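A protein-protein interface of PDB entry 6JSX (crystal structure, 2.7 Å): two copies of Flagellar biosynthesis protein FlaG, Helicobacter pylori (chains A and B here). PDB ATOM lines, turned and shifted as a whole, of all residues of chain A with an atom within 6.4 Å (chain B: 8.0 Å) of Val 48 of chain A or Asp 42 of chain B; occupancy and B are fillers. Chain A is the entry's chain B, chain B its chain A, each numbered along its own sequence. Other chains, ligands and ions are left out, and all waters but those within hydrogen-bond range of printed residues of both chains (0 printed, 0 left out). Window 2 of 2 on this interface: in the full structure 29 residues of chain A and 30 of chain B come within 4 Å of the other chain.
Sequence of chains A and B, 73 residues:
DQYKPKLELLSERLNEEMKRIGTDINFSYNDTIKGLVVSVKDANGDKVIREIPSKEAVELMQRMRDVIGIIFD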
ATOM      1  N   VAL A  38     -11.579 -12.228  14.598  1.00  0.00           N
ATOM      2  CA  VAL A  38     -11.671 -11.223  13.546  1.00  0.00           C
ATOM      3  C   VAL A  38     -12.013 -11.896  12.210  1.00  0.00           C
ATOM      4  O   VAL A  38     -11.497 -12.969  11.899  1.00  0.00           O
ATOM      5  CB  VAL A  38     -10.415 -10.284  13.478  1.00  0.00           C
ATOM      6  CG1 VAL A  38      -9.180 -10.947  14.054  1.00  0.00           C
ATOM      7  CG2 VAL A  38     -10.174  -9.779  12.061  1.00  0.00           C
ATOM      8  N   SER A  39     -12.920 -11.284  11.452  1.00  0.00           N
ATOM      9  CA  SER A  39     -13.350 -11.848  10.177  1.00  0.00           C
ATOM     10  C   SER A  39     -13.405 -10.824   9.046  1.00  0.00           C
ATOM     11  O   SER A  39     -13.651  -9.639   9.270  1.00  0.00           O
ATOM     12  CB  SER A  39     -14.711 -12.545  10.324  1.00  0.00           C
ATOM     13  OG  SER A  39     -15.762 -11.627  10.573  1.00  0.00           O
ATOM     14  N   VAL A  40     -13.151 -11.296   7.831  1.00  0.00           N
ATOM     15  CA  VAL A  40     -13.350 -10.506   6.618  1.00  0.00           C
ATOM     16  C   VAL A  40     -13.981 -11.423   5.573  1.00  0.00           C
ATOM     17  O   VAL A  40     -13.759 -12.628   5.602  1.00  0.00           O
ATOM     18  CB  VAL A  40     -12.021  -9.916   6.082  1.00  0.00           C
ATOM     19  CG1 VAL A  40     -11.433  -8.923   7.082  1.00  0.00           C
ATOM     20  CG2 VAL A  40     -11.022 -11.025   5.798  1.00  0.00           C
ATOM     21  N   LYS A  41     -14.782 -10.857   4.674  1.00  0.00           N
ATOM     22  CA  LYS A  41     -15.409 -11.624   3.595  1.00  0.00           C
ATOM     23  C   LYS A  41     -14.443 -11.838   2.440  1.00  0.00           C
ATOM     24  O   LYS A  41     -13.784 -10.898   1.993  1.00  0.00           O
ATOM     25  CB  LYS A  41     -16.659 -10.903   3.057  1.00  0.00           C
ATOM     26  CG  LYS A  41     -17.683 -10.492   4.116  1.00  0.00           C
ATOM     27  CD  LYS A  41     -18.949 -11.338   4.078  1.00  0.00           C
ATOM     28  CE  LYS A  41     -19.745 -11.193   5.378  1.00  0.00           C
ATOM     29  NZ  LYS A  41     -20.182  -9.792   5.663  1.00  0.00           N
ATOM     30  N   ASP A  42     -14.366 -13.067   1.941  1.00  0.00           N
ATOM     31  CA  ASP A  42     -13.647 -13.304   0.694  1.00  0.00           C
ATOM     32  C   ASP A  42     -14.490 -12.875  -0.507  1.00  0.00           C
ATOM     33  O   ASP A  42     -15.564 -12.287  -0.356  1.00  0.00           O
ATOM     34  CB  ASP A  42     -13.195 -14.765   0.565  1.00  0.00           C
ATOM     35  CG  ASP A  42     -14.352 -15.767   0.648  1.00  0.00           C
ATOM     36  OD1 ASP A  42     -15.457 -15.510   0.112  1.00  0.00           O
ATOM     37  OD2 ASP A  42     -14.142 -16.837   1.256  1.00  0.00           O
ATOM     38  N   ALA A  43     -14.003 -13.186  -1.700  1.00  0.00           N
ATOM     39  CA  ALA A  43     -14.698 -12.843  -2.935  1.00  0.00           C
ATOM     40  C   ALA A  43     -16.138 -13.364  -3.014  1.00  0.00           C
ATOM     41  O   ALA A  43     -16.991 -12.741  -3.647  1.00  0.00           O
ATOM     42  CB  ALA A  43     -13.907 -13.351  -4.120  1.00  0.00           C
ATOM     43  N   ASP A  46     -17.884 -15.454   1.813  1.00  0.00           N
ATOM     44  CA  ASP A  46     -17.570 -16.362   2.916  1.00  0.00           C
ATOM     45  C   ASP A  46     -16.561 -15.755   3.889  1.00  0.00           C
ATOM     46  O   ASP A  46     -15.507 -15.241   3.497  1.00  0.00           O
ATOM     47  CB  ASP A  46     -17.061 -17.702   2.385  1.00  0.00           C
ATOM     48  CG  ASP A  46     -17.972 -18.281   1.323  1.00  0.00           C
ATOM     49  OD1 ASP A  46     -19.187 -18.397   1.598  1.00  0.00           O
ATOM     50  OD2 ASP A  46     -17.479 -18.597   0.213  1.00  0.00           O
ATOM     51  N   LYS A  47     -16.896 -15.812   5.168  1.00  0.00           N
ATOM     52  CA  LYS A  47     -16.021 -15.242   6.177  1.00  0.00           C
ATOM     53  C   LYS A  47     -14.713 -16.021   6.302  1.00  0.00           C
ATOM     54  O   LYS A  47     -14.710 -17.237   6.489  1.00  0.00           O
ATOM     55  CB  LYS A  47     -16.750 -15.108   7.524  1.00  0.00           C
ATOM     56  CG  LYS A  47     -17.822 -14.014   7.507  1.00  0.00           C
ATOM     57  CD  LYS A  47     -18.978 -14.300   8.451  1.00  0.00           C
ATOM     58  CE  LYS A  47     -18.568 -14.151   9.899  1.00  0.00           C
ATOM     59  NZ  LYS A  47     -19.690 -14.519  10.808  1.00  0.00           N
ATOM     60  N   VAL A  48     -13.613 -15.295   6.130  1.00  0.00           N
ATOM     61  CA  VAL A  48     -12.279 -15.733   6.498  1.00  0.00           C
ATOM     62  C   VAL A  48     -12.103 -15.333   7.962  1.00  0.00           C
ATOM     63  O   VAL A  48     -12.430 -14.218   8.349  1.00  0.00           O
ATOM     64  CB  VAL A  48     -11.220 -14.996   5.669  1.00  0.00           C
ATOM     65  CG1 VAL A  48      -9.821 -15.296   6.188  1.00  0.00           C
ATOM     66  CG2 VAL A  48     -11.354 -15.360   4.209  1.00  0.00           C
ATOM     67  N   ILE A  49     -11.623 -16.240   8.798  1.00  0.00           N
ATOM     68  CA  ILE A  49     -11.576 -15.926  10.211  1.00  0.00           C
ATOM     69  C   ILE A  49     -10.193 -16.193  10.813  1.00  0.00           C
ATOM     70  O   ILE A  49      -9.488 -17.115  10.412  1.00  0.00           O
ATOM     71  CB  ILE A  49     -12.720 -16.644  11.024  1.00  0.00           C
ATOM     72  CG1 ILE A  49     -12.263 -17.990  11.560  1.00  0.00           C
ATOM     73  CG2 ILE A  49     -14.018 -16.795  10.213  1.00  0.00           C
ATOM     74  CD1 ILE A  49     -11.956 -17.954  13.015  1.00  0.00           C
ATOM     75  N   ARG A  50      -9.795 -15.348  11.755  1.00  0.00           N
ATOM     76  CA  ARG A  50      -8.560 -15.546  12.490  1.00  0.00           C
ATOM     77  C   ARG A  50      -8.891 -15.427  13.964  1.00  0.00           C
ATOM     78  O   ARG A  50      -9.661 -14.557  14.375  1.00  0.00           O
ATOM     79  CB  ARG A  50      -7.513 -14.503  12.107  1.00  0.00           C
ATOM     80  CG  ARG A  50      -6.963 -14.625  10.698  1.00  0.00           C
ATOM     81  CD  ARG A  50      -6.311 -15.968  10.463  1.00  0.00           C
ATOM     82  NE  ARG A  50      -5.809 -16.078   9.098  1.00  0.00           N
ATOM     83  CZ  ARG A  50      -6.552 -16.487   8.077  1.00  0.00           C
ATOM     84  NH1 ARG A  50      -6.037 -16.559   6.852  1.00  0.00           N
ATOM     85  NH2 ARG A  50      -7.819 -16.816   8.285  1.00  0.00           N
ATOM     86  N   ASP B  24      -1.884 -15.380  11.097  1.00  0.00           N
ATOM     87  CA  ASP B  24      -1.712 -14.961   9.707  1.00  0.00           C
ATOM     88  C   ASP B  24      -2.535 -13.704   9.400  1.00  0.00           C
ATOM     89  O   ASP B  24      -3.631 -13.785   8.815  1.00  0.00           O
ATOM     90  CB  ASP B  24      -2.075 -16.098   8.738  1.00  0.00           C
ATOM     91  CG  ASP B  24      -1.871 -15.714   7.263  1.00  0.00           C
ATOM     92  OD1 ASP B  24      -2.869 -15.415   6.565  1.00  0.00           O
ATOM     93  OD2 ASP B  24      -0.709 -15.716   6.796  1.00  0.00           O
ATOM     94  N   SER B  39      -3.996  -7.736   5.257  1.00  0.00           N
ATOM     95  CA  SER B  39      -4.298  -8.855   4.382  1.00  0.00           C
ATOM     96  C   SER B  39      -4.143 -10.205   5.059  1.00  0.00           C
ATOM     97  O   SER B  39      -3.180 -10.455   5.784  1.00  0.00           O
ATOM     98  CB  SER B  39      -3.470  -8.794   3.093  1.00  0.00           C
ATOM     99  OG  SER B  39      -2.104  -9.054   3.355  1.00  0.00           O
ATOM    100  N   VAL B  40      -5.122 -11.066   4.788  1.00  0.00           N
ATOM    101  CA  VAL B  40      -5.166 -12.433   5.281  1.00  0.00           C
ATOM    102  C   VAL B  40      -5.407 -13.362   4.086  1.00  0.00           C
ATOM    103  O   VAL B  40      -6.004 -12.951   3.097  1.00  0.00           O
ATOM    104  CB  VAL B  40      -6.298 -12.588   6.324  1.00  0.00           C
ATOM    105  CG1 VAL B  40      -6.029 -11.705   7.523  1.00  0.00           C
ATOM    106  CG2 VAL B  40      -7.623 -12.198   5.730  1.00  0.00           C
ATOM    107  N   LYS B  41      -4.926 -14.599   4.151  1.00  0.00           N
ATOM    108  CA  LYS B  41      -5.221 -15.560   3.081  1.00  0.00           C
ATOM    109  C   LYS B  41      -6.461 -16.374   3.433  1.00  0.00           C
ATOM    110  O   LYS B  41      -6.633 -16.786   4.584  1.00  0.00           O
ATOM    111  CB  LYS B  41      -4.021 -16.474   2.786  1.00  0.00           C
ATOM    112  CG  LYS B  41      -2.829 -15.749   2.143  1.00  0.00           C
ATOM    113  CD  LYS B  41      -1.779 -16.729   1.620  1.00  0.00           C
ATOM    114  CE  LYS B  41      -0.726 -16.033   0.755  1.00  0.00           C
ATOM    115  NZ  LYS B  41       0.114 -15.078   1.538  1.00  0.00           N
ATOM    116  N   ASP B  42      -7.329 -16.592   2.448  1.00  0.00           N
ATOM    117  CA  ASP B  42      -8.587 -17.304   2.681  1.00  0.00           C
ATOM    118  C   ASP B  42      -8.413 -18.821   2.721  1.00  0.00           C
ATOM    119  O   ASP B  42      -7.295 -19.325   2.846  1.00  0.00           O
ATOM    120  CB  ASP B  42      -9.642 -16.916   1.634  1.00  0.00           C
ATOM    121  CG  ASP B  42      -9.331 -17.455   0.240  1.00  0.00           C
ATOM    122  OD1 ASP B  42      -8.203 -17.936   0.007  1.00  0.00           O
ATOM    123  OD2 ASP B  42     -10.222 -17.381  -0.633  1.00  0.00           O
ATOM    124  N   ALA B  43      -9.520 -19.547   2.597  1.00  0.00           N
ATOM    125  CA  ALA B  43      -9.462 -21.004   2.622  1.00  0.00           C
ATOM    126  C   ALA B  43      -8.673 -21.592   1.446  1.00  0.00           C
ATOM    127  O   ALA B  43      -8.106 -22.677   1.557  1.00  0.00           O
ATOM    128  CB  ALA B  43     -10.870 -21.608   2.689  1.00  0.00           C
ATOM    129  N   ASN B  44      -8.614 -20.876   0.329  1.00  0.00           N
ATOM    130  CA  ASN B  44      -7.931 -21.416  -0.847  1.00  0.00           C
ATOM    131  C   ASN B  44      -6.463 -21.012  -0.952  1.00  0.00           C
ATOM    132  O   ASN B  44      -5.749 -21.461  -1.852  1.00  0.00           O
ATOM    133  CB  ASN B  44      -8.699 -21.098  -2.141  1.00  0.00           C
ATOM    134  CG  ASN B  44      -9.876 -22.051  -2.380  1.00  0.00           C
ATOM    135  OD1 ASN B  44     -10.571 -22.464  -1.442  1.00  0.00           O
ATOM    136  ND2 ASN B  44     -10.092 -22.412  -3.644  1.00  0.00           N
ATOM    137  N   GLY B  45      -6.022 -20.173  -0.015  1.00  0.00           N
ATOM    138  CA  GLY B  45      -4.642 -19.720   0.048  1.00  0.00           C
ATOM    139  C   GLY B  45      -4.437 -18.423  -0.696  1.00  0.00           C
ATOM    140  O   GLY B  45      -3.303 -17.998  -0.900  1.00  0.00           O
ATOM    141  N   ASP B  46      -5.545 -17.800  -1.096  1.00  0.00           N
ATOM    142  CA  ASP B  46      -5.535 -16.565  -1.884  1.00  0.00           C
ATOM    143  C   ASP B  46      -5.726 -15.327  -1.007  1.00  0.00           C
ATOM    144  O   ASP B  46      -6.510 -15.352  -0.059  1.00  0.00           O
ATOM    145  CB  ASP B  46      -6.652 -16.601  -2.927  1.00  0.00           C
ATOM    146  CG  ASP B  46      -6.556 -17.796  -3.851  1.00  0.00           C
ATOM    147  OD1 ASP B  46      -5.427 -18.152  -4.259  1.00  0.00           O
ATOM    148  OD2 ASP B  46      -7.618 -18.375  -4.168  1.00  0.00           O
ATOM    149  N   LYS B  47      -5.033 -14.239  -1.331  1.00  0.00           N
ATOM    150  CA  LYS B  47      -5.098 -13.048  -0.488  1.00  0.00           C
ATOM    151  C   LYS B  47      -6.426 -12.313  -0.597  1.00  0.00           C
ATOM    152  O   LYS B  47      -6.892 -12.021  -1.696  1.00  0.00           O
ATOM    153  CB  LYS B  47      -3.954 -12.077  -0.799  1.00  0.00           C
ATOM    154  CG  LYS B  47      -2.581 -12.520  -0.315  1.00  0.00           C
ATOM    155  CD  LYS B  47      -1.576 -11.408  -0.541  1.00  0.00           C
ATOM    156  CE  LYS B  47      -0.148 -11.896  -0.401  1.00  0.00           C
ATOM    157  NZ  LYS B  47       0.806 -10.750  -0.477  1.00  0.00           N
ATOM    158  N   VAL B  48      -7.033 -12.035   0.553  1.00  0.00           N
ATOM    159  CA  VAL B  48      -8.156 -11.108   0.632  1.00  0.00           C
ATOM    160  C   VAL B  48      -7.649  -9.881   1.378  1.00  0.00           C
ATOM    161  O   VAL B  48      -6.967 -10.008   2.400  1.00  0.00           O
ATOM    162  CB  VAL B  48      -9.412 -11.750   1.301  1.00  0.00           C
ATOM    163  CG1 VAL B  48      -9.033 -12.501   2.548  1.00  0.00           C
ATOM    164  CG2 VAL B  48     -10.469 -10.707   1.624  1.00  0.00           C
ATOM    165  N   ARG B  50      -7.990  -5.574   2.736  1.00  0.00           N
ATOM    166  CA  ARG B  50      -8.775  -4.420   3.130  1.00  0.00           C
ATOM    167  C   ARG B  50      -7.844  -3.228   3.196  1.00  0.00           C
ATOM    168  O   ARG B  50      -6.809  -3.282   3.852  1.00  0.00           O
ATOM    169  CB  ARG B  50      -9.426  -4.644   4.491  1.00  0.00           C
ATOM    170  CG  ARG B  50     -10.542  -5.667   4.479  1.00  0.00           C
ATOM    171  CD  ARG B  50     -11.556  -5.397   3.375  1.00  0.00           C
ATOM    172  NE  ARG B  50     -12.723  -6.269   3.499  1.00  0.00           N
ATOM    173  CZ  ARG B  50     -12.953  -7.357   2.761  1.00  0.00           C
ATOM    174  NH1 ARG B  50     -12.106  -7.733   1.807  1.00  0.00           N
ATOM    175  NH2 ARG B  50     -14.051  -8.070   2.967  1.00  0.00           N
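Val 48 of chain A touches three residues of chain B. Asp 42 of chain B touches one residue of chain A. Of the printed residues of chain A, Asp 24 of chain B touches Arg 50. Printed residues of chain A within 4 Å of Arg 50 of chain B: Lys 41. Printed residues of chain B within 4 Å of Lys 41 of chain A: Val 48 (3.3 Å) and Arg 50 (3.0 Å). Printed residues of chain A within 4 Å of Val 40 of chain B: Val 40 (3.6 Å) and Val 48 (3.8 Å). The nearest residue of chain B that does not touch Val 48 of chain A is Val 48 of chain B (4.04 Å). The nearest residue of chain A that does not touch Asp 42 of chain B is Asp 42 of chain A (4.1 Å). The nearest printed residue of chain A that does not touch Arg 50 of chain B is Val 40 of chain A (4.2 Å).
Of the 11 printed residues of chain A, 4 touch a printed residue of chain B. Of the 12 printed residues of chain B, 6 touch a printed residue of chain A. Hydrophobic or aromatic side chains of chain B within 4 Å of the printed part of chain A: Val 40 and Val 48. Among the printed residues, 8 pairs touch across the chains. Among the printed residues, Asp or Glu carboxylates within 4 Å of a Lys or Arg side-chain nitrogen of the other chain: Arg 50 of chain A with Asp 24 of chain B (3.4 Å).
The side-chain carboxylate of Asp 24 of chain B is in hydrogen-bond range of the backbone NH of Lys 41 of chain B. The backbone NH of Val 48 of chain B is in hydrogen-bond range of the backbone carbonyl oxygen of Val 40 of chain B, 2.9 Å away. N of Asn 44 of chain B sits at hydrogen-bond distance from OD1 of Asp 42 of chain B, 3.0 Å away. The side-chain carboxylate (OD1) of Asp 42 of chain B lies within hydrogen-bond range of the backbone NH (N) of Gly 45 of chain B, at 3.1 Å. N of Asp 46 of chain B sits at hydrogen-bond distance from OD1 of Asp 42 of chain B, 2.9 Å away. N of Val 48 of chain A sits at hydrogen-bond distance from O of Val 40 of chain A.
OD1 of Asp 24 of chain B is in salt-bridge range of NH1 of Arg 50 of chain A (3.4 Å). NH2 of Arg 50 of chain B lies within hydrogen-bond range of O of Lys 41 of chain A (3.0 Å). O of Lys 41 of chain B sits close to NH1 of Arg 50 of chain A (2.4 Å).
Val 40 of chain B touches its own counterpart, Val 40 of chain A. Lys 41 of chain A touches Val 48 of chain B, and with the chains exchanged Val 48 of chain A touches Lys 41 of chain B. Lys 41 of chain A touches Arg 50 of chain B, and with the chains exchanged Arg 50 of chain A touches Lys 41 of chain B. Val 48 of chain A touches Val 40 of chain B, but with the chains exchanged Val 40 of chain A does not touch Val 48 of chain B (4.1 Å). Positions printed for both chains: 39, 40, 41, 42, 43, 46, 47, 48 and 50. Of the 8 pairs that touch across the chains among the printed residues, 5 have their exchanged pair printed and touching as well.
Val 40 of chain A touches Val 40 of chain B (CG2 to CG2, 3.6 Å). Lys 41 of chain A touches Val 48 of chain B (O to CG2, 3.3 Å). Val 48 of chain A touches Val 40 of chain B. Lys 41 of chain B touches Val 48 of chain A. CB of Asp 42 of chain B touches CG2 of Val 48 of chain A, at 3.5 Å.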
